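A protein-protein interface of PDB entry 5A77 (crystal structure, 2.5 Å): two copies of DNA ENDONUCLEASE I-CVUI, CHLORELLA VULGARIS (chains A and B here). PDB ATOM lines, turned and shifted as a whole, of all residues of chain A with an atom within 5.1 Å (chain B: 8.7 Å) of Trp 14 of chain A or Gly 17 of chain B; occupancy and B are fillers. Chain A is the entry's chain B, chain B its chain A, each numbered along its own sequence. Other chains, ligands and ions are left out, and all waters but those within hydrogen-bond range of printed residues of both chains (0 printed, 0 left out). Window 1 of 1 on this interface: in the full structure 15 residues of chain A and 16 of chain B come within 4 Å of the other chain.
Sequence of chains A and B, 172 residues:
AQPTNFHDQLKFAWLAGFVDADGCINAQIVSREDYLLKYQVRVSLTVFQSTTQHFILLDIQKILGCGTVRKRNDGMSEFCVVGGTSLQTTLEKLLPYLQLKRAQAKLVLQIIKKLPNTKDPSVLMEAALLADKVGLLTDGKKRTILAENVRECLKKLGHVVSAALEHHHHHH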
ATOM      1  N   LEU A  10      11.130   9.230  -2.491  1.00  0.00           N
ATOM      2  CA  LEU A  10      12.009   9.600  -1.388  1.00  0.00           C
ATOM      3  C   LEU A  10      11.874   8.660  -0.210  1.00  0.00           C
ATOM      4  O   LEU A  10      12.861   8.395   0.477  1.00  0.00           O
ATOM      5  CB  LEU A  10      11.739  11.029  -0.930  1.00  0.00           C
ATOM      6  CG  LEU A  10      12.460  12.134  -1.681  1.00  0.00           C
ATOM      7  CD1 LEU A  10      11.923  13.496  -1.274  1.00  0.00           C
ATOM      8  CD2 LEU A  10      13.944  12.052  -1.373  1.00  0.00           C
ATOM      9  N   LYS A  11      10.650   8.192   0.047  1.00  0.00           N
ATOM     10  CA  LYS A  11      10.406   7.198   1.090  1.00  0.00           C
ATOM     11  C   LYS A  11      11.003   5.831   0.721  1.00  0.00           C
ATOM     12  O   LYS A  11      11.547   5.129   1.577  1.00  0.00           O
ATOM     13  CB  LYS A  11       8.900   7.056   1.368  1.00  0.00           C
ATOM     14  CG  LYS A  11       8.238   8.311   1.961  1.00  0.00           C
ATOM     15  CD  LYS A  11       8.810   8.607   3.352  1.00  0.00           C
ATOM     16  CE  LYS A  11       8.216   9.852   4.001  1.00  0.00           C
ATOM     17  NZ  LYS A  11       6.783   9.686   4.363  1.00  0.00           N
ATOM     18  N   PHE A  12      10.895   5.456  -0.554  1.00  0.00           N
ATOM     19  CA  PHE A  12      11.425   4.181  -1.033  1.00  0.00           C
ATOM     20  C   PHE A  12      12.957   4.189  -1.023  1.00  0.00           C
ATOM     21  O   PHE A  12      13.591   3.156  -0.813  1.00  0.00           O
ATOM     22  CB  PHE A  12      10.904   3.871  -2.444  1.00  0.00           C
ATOM     23  CG  PHE A  12       9.427   3.568  -2.499  1.00  0.00           C
ATOM     24  CD1 PHE A  12       8.814   2.844  -1.490  1.00  0.00           C
ATOM     25  CD2 PHE A  12       8.652   4.010  -3.562  1.00  0.00           C
ATOM     26  CE1 PHE A  12       7.446   2.568  -1.536  1.00  0.00           C
ATOM     27  CE2 PHE A  12       7.288   3.745  -3.613  1.00  0.00           C
ATOM     28  CZ  PHE A  12       6.684   3.022  -2.598  1.00  0.00           C
ATOM     29  N   ALA A  13      13.545   5.365  -1.233  1.00  0.00           N
ATOM     30  CA  ALA A  13      15.000   5.523  -1.179  1.00  0.00           C
ATOM     31  C   ALA A  13      15.496   5.439   0.269  1.00  0.00           C
ATOM     32  O   ALA A  13      16.494   4.768   0.554  1.00  0.00           O
ATOM     33  CB  ALA A  13      15.419   6.843  -1.814  1.00  0.00           C
ATOM     34  N   TRP A  14      14.798   6.118   1.173  1.00  0.00           N
ATOM     35  CA  TRP A  14      15.085   6.027   2.602  1.00  0.00           C
ATOM     36  C   TRP A  14      14.982   4.577   3.059  1.00  0.00           C
ATOM     37  O   TRP A  14      15.876   4.065   3.726  1.00  0.00           O
ATOM     38  CB  TRP A  14      14.128   6.913   3.427  1.00  0.00           C
ATOM     39  CG  TRP A  14      14.298   6.742   4.921  1.00  0.00           C
ATOM     40  CD1 TRP A  14      15.129   7.455   5.738  1.00  0.00           C
ATOM     41  CD2 TRP A  14      13.622   5.786   5.767  1.00  0.00           C
ATOM     42  NE1 TRP A  14      15.020   7.002   7.032  1.00  0.00           N
ATOM     43  CE2 TRP A  14      14.112   5.995   7.076  1.00  0.00           C
ATOM     44  CE3 TRP A  14      12.664   4.799   5.539  1.00  0.00           C
ATOM     45  CZ2 TRP A  14      13.661   5.221   8.156  1.00  0.00           C
ATOM     46  CZ3 TRP A  14      12.220   4.039   6.619  1.00  0.00           C
ATOM     47  CH2 TRP A  14      12.723   4.257   7.910  1.00  0.00           C
ATOM     48  N   LEU A  15      13.886   3.918   2.693  1.00  0.00           N
ATOM     49  CA  LEU A  15      13.652   2.532   3.091  1.00  0.00           C
ATOM     50  C   LEU A  15      14.677   1.592   2.466  1.00  0.00           C
ATOM     51  O   LEU A  15      15.152   0.652   3.109  1.00  0.00           O
ATOM     52  CB  LEU A  15      12.239   2.088   2.713  1.00  0.00           C
ATOM     53  CG  LEU A  15      11.948   0.671   3.201  1.00  0.00           C
ATOM     54  CD1 LEU A  15      12.235   0.578   4.694  1.00  0.00           C
ATOM     55  CD2 LEU A  15      10.514   0.251   2.888  1.00  0.00           C
ATOM     56  N   ALA A  16      15.019   1.842   1.211  1.00  0.00           N
ATOM     57  CA  ALA A  16      16.093   1.090   0.613  1.00  0.00           C
ATOM     58  C   ALA A  16      17.335   1.288   1.462  1.00  0.00           C
ATOM     59  O   ALA A  16      18.056   0.329   1.772  1.00  0.00           O
ATOM     60  CB  ALA A  16      16.332   1.529  -0.819  1.00  0.00           C
ATOM     61  N   GLY A  17      17.566   2.539   1.854  1.00  0.00           N
ATOM     62  CA  GLY A  17      18.695   2.874   2.696  1.00  0.00           C
ATOM     63  C   GLY A  17      18.675   2.046   3.963  1.00  0.00           C
ATOM     64  O   GLY A  17      19.709   1.563   4.420  1.00  0.00           O
ATOM     65  N   PHE A  18      17.481   1.849   4.509  1.00  0.00           N
ATOM     66  CA  PHE A  18      17.326   1.161   5.782  1.00  0.00           C
ATOM     67  C   PHE A  18      17.535  -0.345   5.642  1.00  0.00           C
ATOM     68  O   PHE A  18      18.230  -0.967   6.454  1.00  0.00           O
ATOM     69  CB  PHE A  18      15.945   1.464   6.358  1.00  0.00           C
ATOM     70  CG  PHE A  18      15.876   1.377   7.840  1.00  0.00           C
ATOM     71  CD1 PHE A  18      16.394   2.402   8.632  1.00  0.00           C
ATOM     72  CD2 PHE A  18      15.271   0.292   8.456  1.00  0.00           C
ATOM     73  CE1 PHE A  18      16.311   2.341  10.022  1.00  0.00           C
ATOM     74  CE2 PHE A  18      15.181   0.217   9.850  1.00  0.00           C
ATOM     75  CZ  PHE A  18      15.710   1.242  10.633  1.00  0.00           C
ATOM     76  N   ILE A  56       8.830   2.461  14.147  1.00  0.00           N
ATOM     77  CA  ILE A  56       9.427   2.595  12.812  1.00  0.00           C
ATOM     78  C   ILE A  56       9.001   1.436  11.866  1.00  0.00           C
ATOM     79  O   ILE A  56       8.835   1.643  10.664  1.00  0.00           O
ATOM     80  CB  ILE A  56      10.990   2.696  12.900  1.00  0.00           C
ATOM     81  CG1 ILE A  56      11.585   3.382  11.660  1.00  0.00           C
ATOM     82  CG2 ILE A  56      11.647   1.340  13.157  1.00  0.00           C
ATOM     83  CD1 ILE A  56      11.216   4.856  11.526  1.00  0.00           C
ATOM     84  N   ILE A  60       7.001   1.503   8.285  1.00  0.00           N
ATOM     85  CA  ILE A  60       7.478   0.841   7.082  1.00  0.00           C
ATOM     86  C   ILE A  60       6.338   0.048   6.464  1.00  0.00           C
ATOM     87  O   ILE A  60       6.171   0.025   5.251  1.00  0.00           O
ATOM     88  CB  ILE A  60       8.684  -0.071   7.375  1.00  0.00           C
ATOM     89  CG1 ILE A  60       9.923   0.783   7.668  1.00  0.00           C
ATOM     90  CG2 ILE A  60       8.948  -1.000   6.197  1.00  0.00           C
ATOM     91  CD1 ILE A  60      11.040   0.055   8.373  1.00  0.00           C
ATOM     92  N   ILE A  63       4.029   2.579   4.641  1.00  0.00           N
ATOM     93  CA  ILE A  63       4.669   2.999   3.398  1.00  0.00           C
ATOM     94  C   ILE A  63       4.532   1.933   2.311  1.00  0.00           C
ATOM     95  O   ILE A  63       4.278   2.245   1.146  1.00  0.00           O
ATOM     96  CB  ILE A  63       6.162   3.308   3.618  1.00  0.00           C
ATOM     97  CG1 ILE A  63       6.327   4.645   4.340  1.00  0.00           C
ATOM     98  CG2 ILE A  63       6.921   3.335   2.294  1.00  0.00           C
ATOM     99  CD1 ILE A  63       7.757   5.086   4.454  1.00  0.00           C
ATOM    100  N   GLN B   9      18.648  14.330  -3.772  1.00  0.00           N
ATOM    101  CA  GLN B   9      17.775  14.119  -2.622  1.00  0.00           C
ATOM    102  C   GLN B   9      17.522  12.624  -2.466  1.00  0.00           C
ATOM    103  O   GLN B   9      17.313  12.125  -1.359  1.00  0.00           O
ATOM    104  CB  GLN B   9      16.439  14.869  -2.749  1.00  0.00           C
ATOM    105  CG  GLN B   9      16.467  16.276  -3.378  1.00  0.00           C
ATOM    106  CD  GLN B   9      17.394  17.301  -2.711  1.00  0.00           C
ATOM    107  OE1 GLN B   9      17.996  17.061  -1.659  1.00  0.00           O
ATOM    108  NE2 GLN B   9      17.505  18.466  -3.346  1.00  0.00           N
ATOM    109  N   LEU B  10      17.545  11.906  -3.584  1.00  0.00           N
ATOM    110  CA  LEU B  10      17.381  10.457  -3.547  1.00  0.00           C
ATOM    111  C   LEU B  10      18.515   9.765  -2.813  1.00  0.00           C
ATOM    112  O   LEU B  10      18.281   8.766  -2.130  1.00  0.00           O
ATOM    113  CB  LEU B  10      17.249   9.891  -4.964  1.00  0.00           C
ATOM    114  CG  LEU B  10      15.863   9.987  -5.588  1.00  0.00           C
ATOM    115  CD1 LEU B  10      15.926   9.572  -7.023  1.00  0.00           C
ATOM    116  CD2 LEU B  10      14.958   9.048  -4.821  1.00  0.00           C
ATOM    117  N   LYS B  11      19.707  10.335  -2.952  1.00  0.00           N
ATOM    118  CA  LYS B  11      20.926   9.816  -2.379  1.00  0.00           C
ATOM    119  C   LYS B  11      21.041  10.180  -0.927  1.00  0.00           C
ATOM    120  O   LYS B  11      21.496   9.390  -0.141  1.00  0.00           O
ATOM    121  CB  LYS B  11      22.143  10.368  -3.129  1.00  0.00           C
ATOM    122  CG  LYS B  11      22.451   9.787  -4.501  1.00  0.00           C
ATOM    123  CD  LYS B  11      23.191   8.459  -4.422  1.00  0.00           C
ATOM    124  CE  LYS B  11      24.018   8.140  -5.666  1.00  0.00           C
ATOM    125  NZ  LYS B  11      25.253   7.321  -5.430  1.00  0.00           N
ATOM    126  N   PHE B  12      20.651  11.393  -0.581  1.00  0.00           N
ATOM    127  CA  PHE B  12      20.603  11.872   0.801  1.00  0.00           C
ATOM    128  C   PHE B  12      19.539  11.093   1.590  1.00  0.00           C
ATOM    129  O   PHE B  12      19.759  10.719   2.746  1.00  0.00           O
ATOM    130  CB  PHE B  12      20.288  13.371   0.869  1.00  0.00           C
ATOM    131  CG  PHE B  12      21.365  14.256   0.312  1.00  0.00           C
ATOM    132  CD1 PHE B  12      22.652  13.772   0.106  1.00  0.00           C
ATOM    133  CD2 PHE B  12      21.092  15.586   0.009  1.00  0.00           C
ATOM    134  CE1 PHE B  12      23.659  14.597  -0.411  1.00  0.00           C
ATOM    135  CE2 PHE B  12      22.083  16.414  -0.506  1.00  0.00           C
ATOM    136  CZ  PHE B  12      23.374  15.916  -0.718  1.00  0.00           C
ATOM    137  N   ALA B  13      18.388  10.854   0.961  1.00  0.00           N
ATOM    138  CA  ALA B  13      17.311  10.092   1.601  1.00  0.00           C
ATOM    139  C   ALA B  13      17.767   8.667   1.831  1.00  0.00           C
ATOM    140  O   ALA B  13      17.493   8.071   2.876  1.00  0.00           O
ATOM    141  CB  ALA B  13      16.050  10.109   0.761  1.00  0.00           C
ATOM    142  N   TRP B  14      18.472   8.129   0.839  1.00  0.00           N
ATOM    143  CA  TRP B  14      18.987   6.778   0.930  1.00  0.00           C
ATOM    144  C   TRP B  14      19.941   6.746   2.105  1.00  0.00           C
ATOM    145  O   TRP B  14      19.828   5.898   2.989  1.00  0.00           O
ATOM    146  CB  TRP B  14      19.692   6.347  -0.370  1.00  0.00           C
ATOM    147  CG  TRP B  14      20.347   5.011  -0.245  1.00  0.00           C
ATOM    148  CD1 TRP B  14      19.778   3.791  -0.499  1.00  0.00           C
ATOM    149  CD2 TRP B  14      21.673   4.744   0.192  1.00  0.00           C
ATOM    150  NE1 TRP B  14      20.674   2.787  -0.248  1.00  0.00           N
ATOM    151  CE2 TRP B  14      21.872   3.353   0.177  1.00  0.00           C
ATOM    152  CE3 TRP B  14      22.756   5.556   0.588  1.00  0.00           C
ATOM    153  CZ2 TRP B  14      23.059   2.741   0.539  1.00  0.00           C
ATOM    154  CZ3 TRP B  14      23.942   4.959   0.958  1.00  0.00           C
ATOM    155  CH2 TRP B  14      24.085   3.567   0.935  1.00  0.00           C
ATOM    156  N   LEU B  15      20.856   7.708   2.127  1.00  0.00           N
ATOM    157  CA  LEU B  15      21.877   7.762   3.166  1.00  0.00           C
ATOM    158  C   LEU B  15      21.240   7.956   4.534  1.00  0.00           C
ATOM    159  O   LEU B  15      21.635   7.318   5.511  1.00  0.00           O
ATOM    160  CB  LEU B  15      22.884   8.873   2.875  1.00  0.00           C
ATOM    161  CG  LEU B  15      24.033   8.979   3.874  1.00  0.00           C
ATOM    162  CD1 LEU B  15      24.589   7.591   4.174  1.00  0.00           C
ATOM    163  CD2 LEU B  15      25.130   9.912   3.337  1.00  0.00           C
ATOM    164  N   ALA B  16      20.242   8.827   4.602  1.00  0.00           N
ATOM    165  CA  ALA B  16      19.496   8.996   5.842  1.00  0.00           C
ATOM    166  C   ALA B  16      18.937   7.658   6.326  1.00  0.00           C
ATOM    167  O   ALA B  16      18.977   7.355   7.523  1.00  0.00           O
ATOM    168  CB  ALA B  16      18.386   9.995   5.660  1.00  0.00           C
ATOM    169  N   GLY B  17      18.426   6.859   5.389  1.00  0.00           N
ATOM    170  CA  GLY B  17      17.935   5.536   5.715  1.00  0.00           C
ATOM    171  C   GLY B  17      19.041   4.676   6.303  1.00  0.00           C
ATOM    172  O   GLY B  17      18.833   3.965   7.285  1.00  0.00           O
ATOM    173  N   PHE B  18      20.225   4.747   5.709  1.00  0.00           N
ATOM    174  CA  PHE B  18      21.339   3.929   6.165  1.00  0.00           C
ATOM    175  C   PHE B  18      21.828   4.367   7.554  1.00  0.00           C
ATOM    176  O   PHE B  18      21.970   3.533   8.462  1.00  0.00           O
ATOM    177  CB  PHE B  18      22.475   3.987   5.151  1.00  0.00           C
ATOM    178  CG  PHE B  18      23.374   2.800   5.182  1.00  0.00           C
ATOM    179  CD1 PHE B  18      23.009   1.620   4.528  1.00  0.00           C
ATOM    180  CD2 PHE B  18      24.593   2.857   5.841  1.00  0.00           C
ATOM    181  CE1 PHE B  18      23.841   0.513   4.544  1.00  0.00           C
ATOM    182  CE2 PHE B  18      25.441   1.760   5.864  1.00  0.00           C
ATOM    183  CZ  PHE B  18      25.063   0.579   5.208  1.00  0.00           C
ATOM    184  N   VAL B  19      22.097   5.669   7.705  1.00  0.00           N
ATOM    185  CA  VAL B  19      22.412   6.271   9.007  1.00  0.00           C
ATOM    186  C   VAL B  19      21.373   5.867  10.078  1.00  0.00           C
ATOM    187  O   VAL B  19      21.733   5.383  11.156  1.00  0.00           O
ATOM    188  CB  VAL B  19      22.474   7.830   8.918  1.00  0.00           C
ATOM    189  CG1 VAL B  19      22.514   8.458  10.305  1.00  0.00           C
ATOM    190  CG2 VAL B  19      23.662   8.294   8.099  1.00  0.00           C
ATOM    191  N   ASP B  20      20.092   6.056   9.778  1.00  0.00           N
ATOM    192  CA  ASP B  20      19.034   5.713  10.732  1.00  0.00           C
ATOM    193  C   ASP B  20      19.107   4.265  11.201  1.00  0.00           C
ATOM    194  O   ASP B  20      18.871   3.973  12.372  1.00  0.00           O
ATOM    195  CB  ASP B  20      17.654   5.977  10.126  1.00  0.00           C
ATOM    196  CG  ASP B  20      17.087   7.301  10.553  1.00  0.00           C
ATOM    197  OD1 ASP B  20      17.550   7.813  11.593  1.00  0.00           O
ATOM    198  OD2 ASP B  20      16.192   7.831   9.862  1.00  0.00           O
ATOM    199  N   ALA B  21      19.433   3.364  10.276  1.00  0.00           N
ATOM    200  CA  ALA B  21      19.557   1.948  10.599  1.00  0.00           C
ATOM    201  C   ALA B  21      20.875   1.629  11.284  1.00  0.00           C
ATOM    202  O   ALA B  21      20.912   0.900  12.276  1.00  0.00           O
ATOM    203  CB  ALA B  21      19.406   1.094   9.349  1.00  0.00           C
ATOM    204  N   ASP B  22      21.971   2.106  10.691  1.00  0.00           N
ATOM    205  CA  ASP B  22      23.320   1.711  11.113  1.00  0.00           C
ATOM    206  C   ASP B  22      24.342   2.794  11.470  1.00  0.00           C
ATOM    207  O   ASP B  22      25.504   2.503  11.489  1.00  0.00           O
ATOM    208  CB  ASP B  22      23.951   0.856  10.017  1.00  0.00           C
ATOM    209  CG  ASP B  22      24.105  -0.552  10.409  1.00  0.00           C
ATOM    210  OD1 ASP B  22      24.066  -0.837  11.623  1.00  0.00           O
ATOM    211  OD2 ASP B  22      24.286  -1.373   9.496  1.00  0.00           O
ATOM    212  N   GLY B  23      23.929   4.012  11.748  1.00  0.00           N
ATOM    213  CA  GLY B  23      24.891   5.066  11.979  1.00  0.00           C
ATOM    214  C   GLY B  23      25.052   5.421  13.450  1.00  0.00           C
ATOM    215  O   GLY B  23      24.785   4.628  14.353  1.00  0.00           O
ATOM    216  N   VAL B  47      29.421   5.852  10.416  1.00  0.00           N
ATOM    217  CA  VAL B  47      28.710   4.752   9.770  1.00  0.00           C
ATOM    218  C   VAL B  47      29.580   3.494   9.716  1.00  0.00           C
ATOM    219  O   VAL B  47      30.740   3.545   9.314  1.00  0.00           O
ATOM    220  CB  VAL B  47      28.245   5.144   8.348  1.00  0.00           C
ATOM    221  CG1 VAL B  47      27.722   3.940   7.599  1.00  0.00           C
ATOM    222  CG2 VAL B  47      27.173   6.214   8.412  1.00  0.00           C
ATOM    223  N   LEU B  94      21.125  15.525   5.711  1.00  0.00           N
ATOM    224  CA  LEU B  94      20.369  14.352   6.162  1.00  0.00           C
ATOM    225  C   LEU B  94      19.172  14.696   7.058  1.00  0.00           C
ATOM    226  O   LEU B  94      18.343  13.845   7.348  1.00  0.00           O
ATOM    227  CB  LEU B  94      21.287  13.392   6.926  1.00  0.00           C
ATOM    228  CG  LEU B  94      22.651  13.027   6.345  1.00  0.00           C
ATOM    229  CD1 LEU B  94      23.399  12.102   7.295  1.00  0.00           C
ATOM    230  CD2 LEU B  94      22.485  12.379   4.978  1.00  0.00           C
ATOM    231  N   PRO B  96      16.417  16.614   6.663  1.00  0.00           N
ATOM    232  CA  PRO B  96      15.032  16.444   6.198  1.00  0.00           C
ATOM    233  C   PRO B  96      14.569  14.984   6.134  1.00  0.00           C
ATOM    234  O   PRO B  96      13.367  14.746   6.142  1.00  0.00           O
ATOM    235  CB  PRO B  96      15.053  17.053   4.791  1.00  0.00           C
ATOM    236  CG  PRO B  96      16.236  17.982   4.781  1.00  0.00           C
ATOM    237  CD  PRO B  96      17.249  17.334   5.673  1.00  0.00           C
ATOM    238  N   TYR B  97      15.490  14.026   6.080  1.00  0.00           N
ATOM    239  CA  TYR B  97      15.093  12.632   5.861  1.00  0.00           C
ATOM    240  C   TYR B  97      15.279  11.736   7.083  1.00  0.00           C
ATOM    241  O   TYR B  97      14.603  10.720   7.214  1.00  0.00           O
ATOM    242  CB  TYR B  97      15.858  12.056   4.668  1.00  0.00           C
ATOM    243  CG  TYR B  97      15.750  12.947   3.462  1.00  0.00           C
ATOM    244  CD1 TYR B  97      14.550  13.053   2.768  1.00  0.00           C
ATOM    245  CD2 TYR B  97      16.827  13.718   3.044  1.00  0.00           C
ATOM    246  CE1 TYR B  97      14.432  13.888   1.677  1.00  0.00           C
ATOM    247  CE2 TYR B  97      16.721  14.556   1.951  1.00  0.00           C
ATOM    248  CZ  TYR B  97      15.519  14.636   1.270  1.00  0.00           C
ATOM    249  OH  TYR B  97      15.395  15.467   0.182  1.00  0.00           O
ATOM    250  N   LEU B  98      16.187  12.109   7.976  1.00  0.00           N
ATOM    251  CA  LEU B  98      16.358  11.359   9.215  1.00  0.00           C
ATOM    252  C   LEU B  98      15.046  11.217   9.989  1.00  0.00           C
ATOM    253  O   LEU B  98      14.243  12.153  10.076  1.00  0.00           O
ATOM    254  CB  LEU B  98      17.408  12.024  10.105  1.00  0.00           C
ATOM    255  CG  LEU B  98      18.879  11.875   9.712  1.00  0.00           C
ATOM    256  CD1 LEU B  98      19.723  12.815  10.537  1.00  0.00           C
ATOM    257  CD2 LEU B  98      19.330  10.444   9.906  1.00  0.00           C
ATOM    258  N   GLN B  99      14.889  10.068  10.610  1.00  0.00           N
ATOM    259  CA  GLN B  99      13.725   9.747  11.366  1.00  0.00           C
ATOM    260  C   GLN B  99      14.101   9.345  12.739  1.00  0.00           C
ATOM    261  O   GLN B  99      13.864  10.045  13.677  1.00  0.00           O
ATOM    262  CB  GLN B  99      13.051   8.565  10.730  1.00  0.00           C
ATOM    263  CG  GLN B  99      12.460   8.892   9.398  1.00  0.00           C
ATOM    264  CD  GLN B  99      11.247   9.708   9.565  1.00  0.00           C
ATOM    265  OE1 GLN B  99      10.535   9.566  10.543  1.00  0.00           O
ATOM    266  NE2 GLN B  99      10.993  10.570   8.619  1.00  0.00           N
ATOM    267  N   LEU B 100      14.692   8.180  12.836  1.00  0.00           N
ATOM    268  CA  LEU B 100      15.106   7.588  14.100  1.00  0.00           C
ATOM    269  C   LEU B 100      16.161   8.383  14.847  1.00  0.00           C
ATOM    270  O   LEU B 100      16.333   8.201  16.055  1.00  0.00           O
ATOM    271  CB  LEU B 100      15.633   6.175  13.852  1.00  0.00           C
ATOM    272  CG  LEU B 100      14.536   5.212  13.422  1.00  0.00           C
ATOM    273  CD1 LEU B 100      15.076   3.791  13.227  1.00  0.00           C
ATOM    274  CD2 LEU B 100      13.408   5.256  14.452  1.00  0.00           C
ATOM    275  N   LYS B 101      16.876   9.255  14.142  1.00  0.00           N
ATOM    276  CA  LYS B 101      17.981   9.956  14.774  1.00  0.00           C
ATOM    277  C   LYS B 101      17.942  11.476  14.577  1.00  0.00           C
ATOM    278  O   LYS B 101      18.931  12.156  14.816  1.00  0.00           O
ATOM    279  CB  LYS B 101      19.312   9.380  14.269  1.00  0.00           C
ATOM    280  CG  LYS B 101      19.630   8.017  14.875  1.00  0.00           C
ATOM    281  CD  LYS B 101      20.804   7.322  14.194  1.00  0.00           C
ATOM    282  CE  LYS B 101      21.394   6.218  15.075  1.00  0.00           C
ATOM    283  NZ  LYS B 101      20.422   5.148  15.404  1.00  0.00           N
ATOM    284  N   ARG B 102      16.798  12.006  14.158  1.00  0.00           N
ATOM    285  CA  ARG B 102      16.657  13.448  13.983  1.00  0.00           C
ATOM    286  C   ARG B 102      16.990  14.189  15.282  1.00  0.00           C
ATOM    287  O   ARG B 102      17.576  15.277  15.250  1.00  0.00           O
ATOM    288  CB  ARG B 102      15.243  13.806  13.509  1.00  0.00           C
ATOM    289  CG  ARG B 102      15.044  15.290  13.228  1.00  0.00           C
ATOM    290  CD  ARG B 102      13.746  15.567  12.486  1.00  0.00           C
ATOM    291  NE  ARG B 102      13.722  14.956  11.162  1.00  0.00           N
ATOM    292  CZ  ARG B 102      12.612  14.608  10.509  1.00  0.00           C
ATOM    293  NH1 ARG B 102      11.418  14.795  11.061  1.00  0.00           N
ATOM    294  NH2 ARG B 102      12.700  14.053   9.305  1.00  0.00           N
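Of the 12 printed residues of chain A, 6 touch a printed residue of chain B.
Of the 24 printed residues of chain B, 12 touch a printed residue of chain A.
Printed residues of chain B that touch a printed residue of chain A: Gln 9, Leu 10, Ala 13, Trp 14, Ala 16, Gly 17, Phe 18, Asp 20, Ala 21, Tyr 97, Gln 99 and Leu 100.
Hydrophobic or aromatic side chains of chain B that line the printed part of chain A: Leu 10, Ala 13, Trp 14, Phe 18, Ala 21, Tyr 97 and Leu 100.
Along chain B the printed residues that touch a printed residue of chain A span positions 9 to 100.
Among the printed residues, 19 pairs touch across the chains.
OD2 of Asp 20 of chain B lies within hydrogen-bond range of N of Gln 99 of chain B (2.7 Å).
The backbone NH (N) of Leu 100 of chain B sits at hydrogen-bond distance from the side-chain carboxylate (OD1) of Asp 20 of chain B (3.1 Å).
OD1 of Asp 20 of chain B sits at hydrogen-bond distance from N of Lys 101 of chain B, 3.0 Å away.
Ala 13 of chain A touches Trp 14 of chain B, and with the chains exchanged Trp 14 of chain A touches Ala 13 of chain B.
Trp 14 of chain A touches Ala 16 of chain B, but with the chains exchanged Ala 16 of chain A does not touch Trp 14 of chain B (4.01 Å).
Gly 17 of chain B touches its own counterpart, Gly 17 of chain A.
Gly 17 of chain A touches Phe 18 of chain B, and with the chains exchanged Phe 18 of chain A touches Gly 17 of chain B.
9 positions are printed for both chains.
Among the printed residues, pairs that only touch across the chains: Trp 14 of chain A with Ala 13 of chain B (3.2 Å), Phe 18 of chain A with Gly 17 of chain B (3.2 Å), Trp 14 of chain A with Gly 17 of chain B (3.2 Å), Ala 13 of chain A with Trp 14 of chain B (3.2 Å), Gly 17 of chain A with Trp 14 of chain B (3.2 Å), Phe 18 of chain A with Ala 21 of chain B (3.3 Å), Leu 10 of chain A with Gln 9 of chain B (3.4 Å), Ala 13 of chain A with Leu 10 of chain B (3.5 Å), Gly 17 of chain A with Gly 17 of chain B (3.5 Å), Leu 10 of chain A with Ala 13 of chain B (3.6 Å), Phe 18 of chain A with Asp 20 of chain B (3.6 Å), Leu 10 of chain A with Tyr 97 of chain B (3.6 Å), Trp 14 of chain A with Tyr 97 of chain B (3.6 Å), Ile 56 of chain A with Leu 100 of chain B (3.7 Å), Phe 18 of chain A with Leu 100 of chain B (3.7 Å), Trp 14 of chain A with Ala 16 of chain B (3.9 Å) and Trp 14 of chain A with Gln 99 of chain B (3.97 Å).
O of Gly 17 of chain A sits close to N of Phe 18 of chain B.
OD2 of Asp 20 of chain B sits at hydrogen-bond distance from NE1 of Trp 14 of chain A, 3.2 Å away.
Of chain B, only Leu 10 (3.5 Å) and Trp 14 (3.2 Å) come within 4 Å of Ala 13 of chain A.
Of the printed residues of chain A, Leu 10 of chain B touches Ala 13 (3.5 Å).
Lys 11 of chain B touches none of the printed residues of chain A.
Phe 12 of chain B touches none of the printed residues of chain A.
Printed residues of chain A within 4 Å of Asp 20 of chain B: Trp 14 and Phe 18.
Printed residues of chain A within 4 Å of Ala 21 of chain B: Phe 18.
Printed residues of chain A within 4 Å of Tyr 97 of chain B: Leu 10 and Trp 14.
The nearest residue of chain B that does not touch Trp 14 of chain A is Trp 14 of chain B (4.2 Å).
The nearest printed residue of chain A that does not touch Gln 99 of chain B is Ile 56 of chain A (4.2 Å).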
